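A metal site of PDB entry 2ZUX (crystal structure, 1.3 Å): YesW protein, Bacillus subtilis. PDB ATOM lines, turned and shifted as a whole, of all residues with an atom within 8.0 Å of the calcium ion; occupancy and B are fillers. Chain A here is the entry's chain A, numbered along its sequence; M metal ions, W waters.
The backbone carbonyl oxygen (O) of Gly 120 is in hydrogen-bond range of the backbone NH (N) of Glu 129 (2.8 Å).
The side-chain amino group of Lys 157 lies within salt-bridge range of the side-chain carboxylate of Asp 123 (2.5 Å).
N of Gly 126 lies within hydrogen-bond range of OD2 of Asp 121 (2.7 Å).
The side-chain carboxylate (OE1) of Glu 129 sits close to the backbone NH (N) of Val 122, at 2.8 Å.
The side-chain carboxylate of Glu 129 lies close to the side-chain amino group of Lys 157.
N of Gly 124 sits close to OD2 of Asp 121, at 3.5 Å.
The calcium ion is bound by OD1 of Asp 123, 2.3 Å away.
O of Gln 127 is bound to the calcium ion (2.3 Å).
The side-chain carboxylate (OD1) of Asp 125 is bound to the calcium ion (2.4 Å).
The calcium ion is bound by OD1 of Asp 121, at 2.4 Å.
Water W1 is bound to the calcium ion, 2.4 Å away.
OE2 of Glu 129 is bound to the calcium ion (2.5 Å).
The calcium ion is bound by the side-chain carboxylate (OE1) of Glu 129 (2.5 Å).
Water W1 bridges the side-chain carboxylate (OD2) of Asp 125 and the side-chain amino group (NZ) of Lys 157.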
ATOM      1  N   ASN A   9      10.854 -25.318  13.745  1.00  0.00           N
ATOM      2  CA  ASN A   9       9.719 -24.760  14.479  1.00  0.00           C
ATOM      3  C   ASN A   9       8.982 -23.757  13.577  1.00  0.00           C
ATOM      4  O   ASN A   9       9.276 -23.663  12.387  1.00  0.00           O
ATOM      5  CB  ASN A   9      10.138 -24.203  15.852  1.00  0.00           C
ATOM      6  CG  ASN A   9      10.898 -22.871  15.773  1.00  0.00           C
ATOM      7  OD1 ASN A   9      11.018 -22.255  14.708  1.00  0.00           O
ATOM      8  ND2 ASN A   9      11.394 -22.423  16.931  1.00  0.00           N
ATOM      9  N   GLY A 120      22.943 -23.938  11.460  1.00  0.00           N
ATOM     10  CA  GLY A 120      22.515 -25.292  11.738  1.00  0.00           C
ATOM     11  C   GLY A 120      21.783 -25.250  13.054  1.00  0.00           C
ATOM     12  O   GLY A 120      21.984 -24.335  13.855  1.00  0.00           O
ATOM     13  N   ASP A 121      20.891 -26.216  13.257  1.00  0.00           N
ATOM     14  CA  ASP A 121      20.183 -26.352  14.517  1.00  0.00           C
ATOM     15  C   ASP A 121      20.966 -27.369  15.331  1.00  0.00           C
ATOM     16  O   ASP A 121      20.847 -28.578  15.119  1.00  0.00           O
ATOM     17  CB  ASP A 121      18.755 -26.820  14.267  1.00  0.00           C
ATOM     18  CG  ASP A 121      17.964 -26.984  15.532  1.00  0.00           C
ATOM     19  OD1 ASP A 121      18.374 -26.467  16.597  1.00  0.00           O
ATOM     20  OD2 ASP A 121      16.901 -27.638  15.461  1.00  0.00           O
ATOM     21  N   VAL A 122      21.813 -26.878  16.233  1.00  0.00           N
ATOM     22  CA  VAL A 122      22.747 -27.739  16.942  1.00  0.00           C
ATOM     23  C   VAL A 122      22.124 -28.490  18.124  1.00  0.00           C
ATOM     24  O   VAL A 122      22.686 -29.487  18.591  1.00  0.00           O
ATOM     25  CB  VAL A 122      24.021 -27.005  17.411  1.00  0.00           C
ATOM     26  CG1 VAL A 122      24.688 -26.298  16.223  1.00  0.00           C
ATOM     27  CG2 VAL A 122      23.708 -26.027  18.542  1.00  0.00           C
ATOM     28  N   ASP A 123      20.967 -28.019  18.596  1.00  0.00           N
ATOM     29  CA  ASP A 123      20.311 -28.626  19.760  1.00  0.00           C
ATOM     30  C   ASP A 123      18.953 -29.237  19.436  1.00  0.00           C
ATOM     31  O   ASP A 123      18.323 -29.849  20.298  1.00  0.00           O
ATOM     32  CB  ASP A 123      20.253 -27.666  20.953  1.00  0.00           C
ATOM     33  CG  ASP A 123      19.577 -26.333  20.639  1.00  0.00           C
ATOM     34  OD1 ASP A 123      19.240 -26.056  19.469  1.00  0.00           O
ATOM     35  OD2 ASP A 123      19.404 -25.540  21.577  1.00  0.00           O
ATOM     36  N   GLY A 124      18.501 -29.086  18.187  1.00  0.00           N
ATOM     37  CA  GLY A 124      17.327 -29.809  17.704  1.00  0.00           C
ATOM     38  C   GLY A 124      15.964 -29.238  18.074  1.00  0.00           C
ATOM     39  O   GLY A 124      14.976 -29.967  18.046  1.00  0.00           O
ATOM     40  N   ASP A 125      15.920 -27.947  18.405  1.00  0.00           N
ATOM     41  CA  ASP A 125      14.640 -27.333  18.786  1.00  0.00           C
ATOM     42  C   ASP A 125      13.926 -26.654  17.620  1.00  0.00           C
ATOM     43  O   ASP A 125      12.855 -26.065  17.787  1.00  0.00           O
ATOM     44  CB  ASP A 125      14.849 -26.334  19.934  1.00  0.00           C
ATOM     45  CG  ASP A 125      15.649 -25.112  19.526  1.00  0.00           C
ATOM     46  OD1 ASP A 125      16.352 -25.145  18.488  1.00  0.00           O
ATOM     47  OD2 ASP A 125      15.576 -24.089  20.243  1.00  0.00           O
ATOM     48  N   GLY A 126      14.509 -26.739  16.427  1.00  0.00           N
ATOM     49  CA  GLY A 126      13.884 -26.151  15.248  1.00  0.00           C
ATOM     50  C   GLY A 126      14.171 -24.673  15.007  1.00  0.00           C
ATOM     51  O   GLY A 126      13.570 -24.093  14.097  1.00  0.00           O
ATOM     52  N   GLN A 127      15.071 -24.090  15.796  1.00  0.00           N
ATOM     53  CA  GLN A 127      15.565 -22.730  15.574  1.00  0.00           C
ATOM     54  C   GLN A 127      17.055 -22.786  15.258  1.00  0.00           C
ATOM     55  O   GLN A 127      17.812 -23.461  15.955  1.00  0.00           O
ATOM     56  CB  GLN A 127      15.324 -21.851  16.814  1.00  0.00           C
ATOM     57  CG  GLN A 127      15.913 -20.451  16.714  1.00  0.00           C
ATOM     58  CD  GLN A 127      15.711 -19.641  17.961  1.00  0.00           C
ATOM     59  OE1 GLN A 127      14.608 -19.160  18.219  1.00  0.00           O
ATOM     60  NE2 GLN A 127      16.774 -19.464  18.737  1.00  0.00           N
ATOM     61  N   TYR A 128      17.467 -22.089  14.213  1.00  0.00           N
ATOM     62  CA  TYR A 128      18.877 -22.108  13.805  1.00  0.00           C
ATOM     63  C   TYR A 128      19.797 -21.375  14.773  1.00  0.00           C
ATOM     64  O   TYR A 128      19.436 -20.332  15.323  1.00  0.00           O
ATOM     65  CB  TYR A 128      19.045 -21.488  12.417  1.00  0.00           C
ATOM     66  CG  TYR A 128      18.464 -22.328  11.308  1.00  0.00           C
ATOM     67  CD1 TYR A 128      19.001 -23.585  11.021  1.00  0.00           C
ATOM     68  CD2 TYR A 128      17.401 -21.872  10.554  1.00  0.00           C
ATOM     69  CE1 TYR A 128      18.473 -24.367  10.018  1.00  0.00           C
ATOM     70  CE2 TYR A 128      16.873 -22.646   9.536  1.00  0.00           C
ATOM     71  CZ  TYR A 128      17.402 -23.891   9.269  1.00  0.00           C
ATOM     72  OH  TYR A 128      16.877 -24.661   8.259  1.00  0.00           O
ATOM     73  N   GLU A 129      20.978 -21.950  14.940  1.00  0.00           N
ATOM     74  CA  GLU A 129      22.131 -21.279  15.519  1.00  0.00           C
ATOM     75  C   GLU A 129      22.988 -20.719  14.380  1.00  0.00           C
ATOM     76  O   GLU A 129      22.938 -21.227  13.253  1.00  0.00           O
ATOM     77  CB  GLU A 129      22.975 -22.256  16.342  1.00  0.00           C
ATOM     78  CG  GLU A 129      22.464 -22.562  17.738  1.00  0.00           C
ATOM     79  CD  GLU A 129      21.110 -23.259  17.755  1.00  0.00           C
ATOM     80  OE1 GLU A 129      20.981 -24.374  17.200  1.00  0.00           O
ATOM     81  OE2 GLU A 129      20.164 -22.687  18.344  1.00  0.00           O
ATOM     82  N   LEU A 130      23.752 -19.684  14.676  1.00  0.00           N
ATOM     83  CA  LEU A 130      24.710 -19.111  13.738  1.00  0.00           C
ATOM     84  C   LEU A 130      26.101 -19.644  14.035  1.00  0.00           C
ATOM     85  O   LEU A 130      26.562 -19.608  15.177  1.00  0.00           O
ATOM     86  CB  LEU A 130      24.706 -17.591  13.854  1.00  0.00           C
ATOM     87  CG  LEU A 130      23.531 -16.918  13.144  1.00  0.00           C
ATOM     88  CD1 LEU A 130      23.248 -15.538  13.740  1.00  0.00           C
ATOM     89  CD2 LEU A 130      23.766 -16.851  11.633  1.00  0.00           C
ATOM     90  N   TYR A 156      26.768 -19.325  17.997  1.00  0.00           N
ATOM     91  CA  TYR A 156      25.873 -18.478  18.802  1.00  0.00           C
ATOM     92  C   TYR A 156      24.425 -18.900  18.652  1.00  0.00           C
ATOM     93  O   TYR A 156      23.954 -19.186  17.553  1.00  0.00           O
ATOM     94  CB  TYR A 156      25.973 -17.014  18.388  1.00  0.00           C
ATOM     95  CG  TYR A 156      27.310 -16.402  18.673  1.00  0.00           C
ATOM     96  CD1 TYR A 156      27.565 -15.777  19.900  1.00  0.00           C
ATOM     97  CD2 TYR A 156      28.342 -16.446  17.728  1.00  0.00           C
ATOM     98  CE1 TYR A 156      28.802 -15.242  20.182  1.00  0.00           C
ATOM     99  CE2 TYR A 156      29.571 -15.906  17.999  1.00  0.00           C
ATOM    100  CZ  TYR A 156      29.799 -15.298  19.230  1.00  0.00           C
ATOM    101  OH  TYR A 156      31.041 -14.762  19.499  1.00  0.00           O
ATOM    102  N   LYS A 157      23.699 -18.922  19.778  1.00  0.00           N
ATOM    103  CA  LYS A 157      22.255 -18.934  19.722  1.00  0.00           C
ATOM    104  C   LYS A 157      21.780 -17.542  19.375  1.00  0.00           C
ATOM    105  O   LYS A 157      22.495 -16.569  19.589  1.00  0.00           O
ATOM    106  CB  LYS A 157      21.669 -19.372  21.063  1.00  0.00           C
ATOM    107  CG  LYS A 157      21.902 -20.833  21.358  1.00  0.00           C
ATOM    108  CD  LYS A 157      21.242 -21.253  22.670  1.00  0.00           C
ATOM    109  CE  LYS A 157      20.953 -22.740  22.666  1.00  0.00           C
ATOM    110  NZ  LYS A 157      19.901 -23.082  21.663  1.00  0.00           N
ATOM    111  N   LEU A 158      20.557 -17.438  18.846  1.00  0.00           N
ATOM    112  CA  LEU A 158      20.030 -16.121  18.469  1.00  0.00           C
ATOM    113  C   LEU A 158      19.859 -15.193  19.677  1.00  0.00           C
ATOM    114  O   LEU A 158      19.870 -13.976  19.534  1.00  0.00           O
ATOM    115  CB  LEU A 158      18.716 -16.254  17.685  1.00  0.00           C
ATOM    116  CG  LEU A 158      18.786 -17.106  16.408  1.00  0.00           C
ATOM    117  CD1 LEU A 158      17.483 -16.941  15.629  1.00  0.00           C
ATOM    118  CD2 LEU A 158      20.000 -16.754  15.528  1.00  0.00           C
ATOM    119  N   LEU A 163      28.021 -20.583  22.408  1.00  0.00           N
ATOM    120  CA  LEU A 163      28.114 -21.999  22.763  1.00  0.00           C
ATOM    121  C   LEU A 163      29.535 -22.510  22.859  1.00  0.00           C
ATOM    122  O   LEU A 163      29.844 -23.322  23.724  1.00  0.00           O
ATOM    123  CB  LEU A 163      27.286 -22.852  21.806  1.00  0.00           C
ATOM    124  CG  LEU A 163      25.803 -22.504  21.743  1.00  0.00           C
ATOM    125  CD1 LEU A 163      25.106 -23.394  20.738  1.00  0.00           C
ATOM    126  CD2 LEU A 163      25.132 -22.615  23.117  1.00  0.00           C
ATOM    127  N   GLY A 190      18.937 -35.229  14.128  1.00  0.00           N
ATOM    128  CA  GLY A 190      18.188 -33.987  14.353  1.00  0.00           C
ATOM    129  C   GLY A 190      19.020 -32.810  14.816  1.00  0.00           C
ATOM    130  O   GLY A 190      18.486 -31.706  15.010  1.00  0.00           O
HETATM  131 CA    CA M   1      18.541 -24.489  17.925  1.00  0.00          CA
HETATM  132  O   HOH W   1      17.623 -22.822  19.371  1.00  0.00           O
